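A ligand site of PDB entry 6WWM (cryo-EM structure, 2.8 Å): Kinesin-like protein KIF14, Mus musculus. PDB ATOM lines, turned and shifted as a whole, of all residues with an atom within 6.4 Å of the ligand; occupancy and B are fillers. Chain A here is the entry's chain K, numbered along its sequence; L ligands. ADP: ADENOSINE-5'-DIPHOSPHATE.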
ATOM      1  N   ARG A  14      23.603  36.669   3.552  1.00  0.00           N
ATOM      2  CA  ARG A  14      24.079  35.452   2.922  1.00  0.00           C
ATOM      3  C   ARG A  14      23.051  34.994   1.907  1.00  0.00           C
ATOM      4  O   ARG A  14      21.931  34.635   2.274  1.00  0.00           O
ATOM      5  CB  ARG A  14      24.332  34.357   3.971  1.00  0.00           C
ATOM      6  CG  ARG A  14      25.379  33.340   3.595  1.00  0.00           C
ATOM      7  CD  ARG A  14      24.848  32.215   2.722  1.00  0.00           C
ATOM      8  NE  ARG A  14      23.817  31.439   3.388  1.00  0.00           N
ATOM      9  CZ  ARG A  14      24.032  30.587   4.394  1.00  0.00           C
ATOM     10  NH1 ARG A  14      23.011  29.934   4.919  1.00  0.00           N
ATOM     11  NH2 ARG A  14      25.255  30.389   4.867  1.00  0.00           N
ATOM     12  N   VAL A  15      23.434  34.989   0.635  1.00  0.00           N
ATOM     13  CA  VAL A  15      22.556  34.554  -0.452  1.00  0.00           C
ATOM     14  C   VAL A  15      22.742  33.052  -0.615  1.00  0.00           C
ATOM     15  O   VAL A  15      23.864  32.557  -0.714  1.00  0.00           O
ATOM     16  CB  VAL A  15      22.881  35.286  -1.759  1.00  0.00           C
ATOM     17  CG1 VAL A  15      21.766  35.067  -2.776  1.00  0.00           C
ATOM     18  CG2 VAL A  15      23.084  36.743  -1.507  1.00  0.00           C
ATOM     19  N   ARG A  16      21.626  32.338  -0.675  1.00  0.00           N
ATOM     20  CA  ARG A  16      21.685  30.897  -0.791  1.00  0.00           C
ATOM     21  C   ARG A  16      21.905  30.511  -2.257  1.00  0.00           C
ATOM     22  O   ARG A  16      21.523  31.247  -3.159  1.00  0.00           O
ATOM     23  CB  ARG A  16      20.410  30.258  -0.240  1.00  0.00           C
ATOM     24  CG  ARG A  16      19.357  29.832  -1.253  1.00  0.00           C
ATOM     25  CD  ARG A  16      18.072  29.393  -0.597  1.00  0.00           C
ATOM     26  NE  ARG A  16      16.931  29.475  -1.491  1.00  0.00           N
ATOM     27  CZ  ARG A  16      16.570  28.537  -2.365  1.00  0.00           C
ATOM     28  NH1 ARG A  16      17.263  27.409  -2.500  1.00  0.00           N
ATOM     29  NH2 ARG A  16      15.503  28.729  -3.121  1.00  0.00           N
ATOM     30  N   PRO A  17      22.513  29.351  -2.504  1.00  0.00           N
ATOM     31  CA  PRO A  17      22.633  28.878  -3.885  1.00  0.00           C
ATOM     32  C   PRO A  17      21.398  28.088  -4.299  1.00  0.00           C
ATOM     33  O   PRO A  17      20.656  27.614  -3.436  1.00  0.00           O
ATOM     34  CB  PRO A  17      23.880  28.007  -3.833  1.00  0.00           C
ATOM     35  CG  PRO A  17      23.789  27.384  -2.532  1.00  0.00           C
ATOM     36  CD  PRO A  17      23.246  28.446  -1.612  1.00  0.00           C
ATOM     37  N   PHE A  18      21.199  27.917  -5.601  1.00  0.00           N
ATOM     38  CA  PHE A  18      19.953  27.356  -6.108  1.00  0.00           C
ATOM     39  C   PHE A  18      19.741  25.940  -5.605  1.00  0.00           C
ATOM     40  O   PHE A  18      20.673  25.156  -5.450  1.00  0.00           O
ATOM     41  CB  PHE A  18      19.960  27.356  -7.633  1.00  0.00           C
ATOM     42  CG  PHE A  18      19.408  28.598  -8.253  1.00  0.00           C
ATOM     43  CD1 PHE A  18      18.093  28.947  -8.081  1.00  0.00           C
ATOM     44  CD2 PHE A  18      20.211  29.394  -9.024  1.00  0.00           C
ATOM     45  CE1 PHE A  18      17.595  30.088  -8.660  1.00  0.00           C
ATOM     46  CE2 PHE A  18      19.720  30.527  -9.604  1.00  0.00           C
ATOM     47  CZ  PHE A  18      18.413  30.881  -9.421  1.00  0.00           C
ATOM     48  N   SER A  19      18.473  25.627  -5.352  1.00  0.00           N
ATOM     49  CA  SER A  19      18.058  24.279  -4.970  1.00  0.00           C
ATOM     50  C   SER A  19      17.861  23.426  -6.212  1.00  0.00           C
ATOM     51  O   SER A  19      17.920  23.906  -7.351  1.00  0.00           O
ATOM     52  CB  SER A  19      16.795  24.353  -4.127  1.00  0.00           C
ATOM     53  OG  SER A  19      15.838  25.220  -4.717  1.00  0.00           O
ATOM     54  N   SER A  59      27.394  33.207  -1.409  1.00  0.00           N
ATOM     55  CA  SER A  59      27.397  31.752  -1.425  1.00  0.00           C
ATOM     56  C   SER A  59      26.552  31.181  -2.552  1.00  0.00           C
ATOM     57  O   SER A  59      25.853  30.185  -2.350  1.00  0.00           O
ATOM     58  CB  SER A  59      26.934  31.226  -0.080  1.00  0.00           C
ATOM     59  OG  SER A  59      26.520  29.883  -0.179  1.00  0.00           O
ATOM     60  N   GLU A  62      30.369  27.804  -5.933  1.00  0.00           N
ATOM     61  CA  GLU A  62      31.553  27.496  -5.146  1.00  0.00           C
ATOM     62  C   GLU A  62      32.797  28.265  -5.567  1.00  0.00           C
ATOM     63  O   GLU A  62      33.608  28.603  -4.706  1.00  0.00           O
ATOM     64  CB  GLU A  62      31.820  25.999  -5.210  1.00  0.00           C
ATOM     65  CG  GLU A  62      30.819  25.148  -4.430  1.00  0.00           C
ATOM     66  CD  GLU A  62      29.518  24.910  -5.173  1.00  0.00           C
ATOM     67  OE1 GLU A  62      28.645  24.181  -4.627  1.00  0.00           O
ATOM     68  OE2 GLU A  62      29.341  25.444  -6.284  1.00  0.00           O
ATOM     69  N   TYR A  67      33.788  33.693  -1.892  1.00  0.00           N
ATOM     70  CA  TYR A  67      32.890  32.645  -1.429  1.00  0.00           C
ATOM     71  C   TYR A  67      32.938  32.561   0.088  1.00  0.00           C
ATOM     72  O   TYR A  67      33.941  32.892   0.724  1.00  0.00           O
ATOM     73  CB  TYR A  67      33.267  31.310  -2.045  1.00  0.00           C
ATOM     74  CG  TYR A  67      32.277  30.197  -1.826  1.00  0.00           C
ATOM     75  CD1 TYR A  67      30.991  30.282  -2.325  1.00  0.00           C
ATOM     76  CD2 TYR A  67      32.629  29.059  -1.143  1.00  0.00           C
ATOM     77  CE1 TYR A  67      30.084  29.275  -2.130  1.00  0.00           C
ATOM     78  CE2 TYR A  67      31.726  28.029  -0.939  1.00  0.00           C
ATOM     79  CZ  TYR A  67      30.451  28.149  -1.437  1.00  0.00           C
ATOM     80  OH  TYR A  67      29.550  27.134  -1.242  1.00  0.00           O
ATOM     81  N   ALA A  68      31.826  32.100   0.678  1.00  0.00           N
ATOM     82  CA  ALA A  68      31.626  32.108   2.117  1.00  0.00           C
ATOM     83  C   ALA A  68      31.244  30.715   2.565  1.00  0.00           C
ATOM     84  O   ALA A  68      30.073  30.327   2.520  1.00  0.00           O
ATOM     85  CB  ALA A  68      30.579  33.123   2.513  1.00  0.00           C
ATOM     86  N   GLN A  70      30.974  27.907   5.696  1.00  0.00           N
ATOM     87  CA  GLN A  70      30.479  28.033   7.058  1.00  0.00           C
ATOM     88  C   GLN A  70      31.564  28.503   8.014  1.00  0.00           C
ATOM     89  O   GLN A  70      31.295  29.283   8.938  1.00  0.00           O
ATOM     90  CB  GLN A  70      29.905  26.705   7.515  1.00  0.00           C
ATOM     91  CG  GLN A  70      28.741  26.200   6.689  1.00  0.00           C
ATOM     92  CD  GLN A  70      27.419  26.721   7.155  1.00  0.00           C
ATOM     93  OE1 GLN A  70      27.272  27.910   7.444  1.00  0.00           O
ATOM     94  NE2 GLN A  70      26.430  25.839   7.231  1.00  0.00           N
ATOM     95  N   GLY A  97      14.909  35.804   8.065  1.00  0.00           N
ATOM     96  CA  GLY A  97      14.738  35.195   6.770  1.00  0.00           C
ATOM     97  C   GLY A  97      13.427  34.472   6.644  1.00  0.00           C
ATOM     98  O   GLY A  97      12.975  33.836   7.599  1.00  0.00           O
ATOM     99  N   GLN A  98      12.690  34.538   5.500  1.00  0.00           N
ATOM    100  CA  GLN A  98      11.403  33.871   5.257  1.00  0.00           C
ATOM    101  C   GLN A  98      11.734  32.439   4.875  1.00  0.00           C
ATOM    102  O   GLN A  98      12.882  32.100   4.547  1.00  0.00           O
ATOM    103  CB  GLN A  98      10.651  34.600   4.151  1.00  0.00           C
ATOM    104  CG  GLN A  98      10.831  36.096   4.196  1.00  0.00           C
ATOM    105  CD  GLN A  98       9.510  36.800   4.194  1.00  0.00           C
ATOM    106  OE1 GLN A  98       8.461  36.182   4.370  1.00  0.00           O
ATOM    107  NE2 GLN A  98       9.532  38.104   3.987  1.00  0.00           N
ATOM    108  N   THR A  99      10.719  31.657   4.899  1.00  0.00           N
ATOM    109  CA  THR A  99      10.833  30.236   4.613  1.00  0.00           C
ATOM    110  C   THR A  99      11.344  30.012   3.202  1.00  0.00           C
ATOM    111  O   THR A  99      10.707  30.412   2.221  1.00  0.00           O
ATOM    112  CB  THR A  99       9.491  29.535   4.839  1.00  0.00           C
ATOM    113  OG1 THR A  99       9.643  28.128   4.604  1.00  0.00           O
ATOM    114  CG2 THR A  99       8.381  30.078   3.928  1.00  0.00           C
ATOM    115  N   GLY A 100      12.515  29.389   3.104  1.00  0.00           N
ATOM    116  CA  GLY A 100      13.179  29.158   1.840  1.00  0.00           C
ATOM    117  C   GLY A 100      14.245  30.194   1.573  1.00  0.00           C
ATOM    118  O   GLY A 100      14.306  30.749   0.479  1.00  0.00           O
ATOM    119  N   SER A 101      15.078  30.447   2.578  1.00  0.00           N
ATOM    120  CA  SER A 101      16.138  31.451   2.479  1.00  0.00           C
ATOM    121  C   SER A 101      17.487  30.931   2.956  1.00  0.00           C
ATOM    122  O   SER A 101      18.520  31.514   2.596  1.00  0.00           O
ATOM    123  CB  SER A 101      15.762  32.694   3.279  1.00  0.00           C
ATOM    124  OG  SER A 101      14.792  33.470   2.593  1.00  0.00           O
ATOM    125  N   GLY A 102      17.525  29.878   3.771  1.00  0.00           N
ATOM    126  CA  GLY A 102      18.761  29.308   4.236  1.00  0.00           C
ATOM    127  C   GLY A 102      19.154  29.779   5.617  1.00  0.00           C
ATOM    128  O   GLY A 102      20.317  30.118   5.859  1.00  0.00           O
ATOM    129  N   LYS A 103      18.189  29.777   6.528  1.00  0.00           N
ATOM    130  CA  LYS A 103      18.399  30.205   7.909  1.00  0.00           C
ATOM    131  C   LYS A 103      18.733  29.045   8.831  1.00  0.00           C
ATOM    132  O   LYS A 103      19.637  29.153   9.653  1.00  0.00           O
ATOM    133  CB  LYS A 103      17.157  30.929   8.408  1.00  0.00           C
ATOM    134  CG  LYS A 103      17.124  31.207   9.883  1.00  0.00           C
ATOM    135  CD  LYS A 103      16.316  32.455  10.230  1.00  0.00           C
ATOM    136  CE  LYS A 103      14.822  32.275   9.996  1.00  0.00           C
ATOM    137  NZ  LYS A 103      14.171  31.546  11.089  1.00  0.00           N
ATOM    138  N   SER A 104      18.023  27.917   8.703  1.00  0.00           N
ATOM    139  CA  SER A 104      18.354  26.750   9.514  1.00  0.00           C
ATOM    140  C   SER A 104      19.709  26.184   9.125  1.00  0.00           C
ATOM    141  O   SER A 104      20.443  25.668   9.975  1.00  0.00           O
ATOM    142  CB  SER A 104      17.265  25.683   9.358  1.00  0.00           C
ATOM    143  OG  SER A 104      16.036  26.131   9.886  1.00  0.00           O
ATOM    144  N   TYR A 105      20.061  26.283   7.851  1.00  0.00           N
ATOM    145  CA  TYR A 105      21.362  25.821   7.381  1.00  0.00           C
ATOM    146  C   TYR A 105      22.470  26.718   7.915  1.00  0.00           C
ATOM    147  O   TYR A 105      23.628  26.297   8.012  1.00  0.00           O
ATOM    148  CB  TYR A 105      21.405  25.824   5.856  1.00  0.00           C
ATOM    149  CG  TYR A 105      22.631  25.172   5.272  1.00  0.00           C
ATOM    150  CD1 TYR A 105      22.682  23.810   5.072  1.00  0.00           C
ATOM    151  CD2 TYR A 105      23.718  25.927   4.904  1.00  0.00           C
ATOM    152  CE1 TYR A 105      23.809  23.217   4.525  1.00  0.00           C
ATOM    153  CE2 TYR A 105      24.833  25.350   4.359  1.00  0.00           C
ATOM    154  CZ  TYR A 105      24.872  24.003   4.170  1.00  0.00           C
ATOM    155  OH  TYR A 105      25.994  23.432   3.625  1.00  0.00           O
ATOM    156  N   THR A 106      22.123  27.947   8.262  1.00  0.00           N
ATOM    157  CA  THR A 106      23.110  28.937   8.685  1.00  0.00           C
ATOM    158  C   THR A 106      23.441  28.787  10.162  1.00  0.00           C
ATOM    159  O   THR A 106      24.600  28.562  10.524  1.00  0.00           O
ATOM    160  CB  THR A 106      22.586  30.339   8.387  1.00  0.00           C
ATOM    161  OG1 THR A 106      22.266  30.439   6.996  1.00  0.00           O
ATOM    162  CG2 THR A 106      23.623  31.350   8.730  1.00  0.00           C
ATOM    163  N   LEU A 110      23.672  21.292   8.991  1.00  0.00           N
ATOM    164  CA  LEU A 110      23.411  19.873   8.793  1.00  0.00           C
ATOM    165  C   LEU A 110      24.398  19.038   9.595  1.00  0.00           C
ATOM    166  O   LEU A 110      25.395  19.526  10.122  1.00  0.00           O
ATOM    167  CB  LEU A 110      23.514  19.523   7.311  1.00  0.00           C
ATOM    168  CG  LEU A 110      22.404  20.066   6.400  1.00  0.00           C
ATOM    169  CD1 LEU A 110      22.780  19.853   4.953  1.00  0.00           C
ATOM    170  CD2 LEU A 110      21.063  19.409   6.710  1.00  0.00           C
ATOM    171  N   ASN A 214       4.753  26.863   2.503  1.00  0.00           N
ATOM    172  CA  ASN A 214       5.459  25.867   3.309  1.00  0.00           C
ATOM    173  C   ASN A 214       4.805  25.726   4.676  1.00  0.00           C
ATOM    174  O   ASN A 214       4.605  26.720   5.384  1.00  0.00           O
ATOM    175  CB  ASN A 214       6.926  26.264   3.449  1.00  0.00           C
ATOM    176  CG  ASN A 214       7.791  25.156   4.064  1.00  0.00           C
ATOM    177  OD1 ASN A 214       7.292  24.242   4.709  1.00  0.00           O
ATOM    178  ND2 ASN A 214       9.102  25.267   3.865  1.00  0.00           N
ATOM    179  N   THR A 327      19.169  36.092   5.724  1.00  0.00           N
ATOM    180  CA  THR A 327      19.211  35.105   4.669  1.00  0.00           C
ATOM    181  C   THR A 327      18.211  35.470   3.582  1.00  0.00           C
ATOM    182  O   THR A 327      17.052  35.777   3.878  1.00  0.00           O
ATOM    183  CB  THR A 327      18.905  33.724   5.236  1.00  0.00           C
ATOM    184  OG1 THR A 327      17.546  33.679   5.692  1.00  0.00           O
ATOM    185  CG2 THR A 327      19.817  33.435   6.411  1.00  0.00           C
HETATM  186  PB  ADP L   1      15.018  28.027   6.244  1.00  0.00           P
HETATM  187  O1B ADP L   1      15.600  27.394   7.480  1.00  0.00           O
HETATM  188  O2B ADP L   1      13.545  27.770   6.054  1.00  0.00           O
HETATM  189  O3B ADP L   1      15.460  29.448   6.007  1.00  0.00           O
HETATM  190  PA  ADP L   1      15.574  25.609   4.994  1.00  0.00           P
HETATM  191  O1A ADP L   1      16.526  25.035   5.996  1.00  0.00           O
HETATM  192  O2A ADP L   1      14.108  25.235   5.036  1.00  0.00           O
HETATM  193  O3A ADP L   1      15.709  27.210   5.037  1.00  0.00           O
HETATM  194  O5' ADP L   1      16.140  25.253   3.533  1.00  0.00           O
HETATM  195  C5' ADP L   1      17.365  25.851   3.141  1.00  0.00           C
HETATM  196  C4' ADP L   1      18.026  25.069   2.007  1.00  0.00           C
HETATM  197  O4' ADP L   1      18.950  25.902   1.317  1.00  0.00           O
HETATM  198  C3' ADP L   1      18.775  23.841   2.495  1.00  0.00           C
HETATM  199  O3' ADP L   1      18.154  22.650   1.989  1.00  0.00           O
HETATM  200  C2' ADP L   1      20.180  23.992   1.966  1.00  0.00           C
HETATM  201  O2' ADP L   1      20.582  22.842   1.223  1.00  0.00           O
HETATM  202  C1' ADP L   1      20.175  25.218   1.093  1.00  0.00           C
HETATM  203  N9  ADP L   1      21.312  26.101   1.455  1.00  0.00           N
HETATM  204  C8  ADP L   1      21.228  27.152   2.275  1.00  0.00           C
HETATM  205  N7  ADP L   1      22.426  27.760   2.406  1.00  0.00           N
HETATM  206  C5  ADP L   1      23.302  27.075   1.657  1.00  0.00           C
HETATM  207  C6  ADP L   1      24.736  27.179   1.345  1.00  0.00           C
HETATM  208  N6  ADP L   1      25.478  28.167   1.893  1.00  0.00           N
HETATM  209  N1  ADP L   1      25.278  26.276   0.506  1.00  0.00           N
HETATM  210  C2  ADP L   1      24.537  25.287  -0.032  1.00  0.00           C
HETATM  211  N3  ADP L   1      23.225  25.145   0.204  1.00  0.00           N
HETATM  212  C4  ADP L   1      22.562  25.992   1.031  1.00  0.00           C
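An oxygen (O1B) of the ligand is in hydrogen-bond range of the backbone NH of Ser 104, at 2.8 Å. The side-chain hydroxyl (OG) of Ser 104 sits at hydrogen-bond distance from an oxygen (O1B) of the ligand, 2.8 Å away. N of Lys 103 sits at hydrogen-bond distance from O3B of the ligand (2.8 Å). The side-chain hydroxyl of Ser 59 sits at hydrogen-bond distance from a nitrogen (N6) of the ligand (2.9 Å). An oxygen (O3B) of the ligand is in hydrogen-bond range of the backbone NH (N) of Gly 102. A nitrogen (N7) of the ligand is in hydrogen-bond range of the guanidinium group (NH1) of Arg 14 (3.4 Å).
The backbone carbonyl oxygen of Gly 102 is in hydrogen-bond range of the guanidinium group of Arg 14 (2.9 Å). The side-chain amide nitrogen of Gln 70 sits at hydrogen-bond distance from the backbone carbonyl oxygen of Tyr 105 (2.9 Å). The side-chain hydroxyl (OG) of Ser 101 lies within hydrogen-bond range of the backbone carbonyl oxygen (O) of Gln 98. O of Thr 327 lies close to OG of Ser 101, at 3.5 Å. The side-chain hydroxyl (OG1) of Thr 99 lies within hydrogen-bond range of the side-chain amide nitrogen (ND2) of Asn 214 (3.0 Å).
CG of Pro 17 touches C2 of the ligand (3.3 Å). Gln 98 touches the ligand (O to O3B, 3.98 Å). CA of Thr 99 touches O2B of the ligand (3.9 Å). Gly 100 touches the ligand. N of Ser 101 touches O3B of the ligand, 3.6 Å away. Tyr 105 touches the ligand (CD2 to N7, 3.4 Å). 11 residues have an atom within 4 Å of the ligand: Arg 14, Pro 17, Ser 59, Gln 98, Thr 99, Gly 100, Ser 101, Gly 102, Lys 103, Ser 104 and Tyr 105. The nearest printed residue that does not touch the ligand is Arg 16 (4.1 Å).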
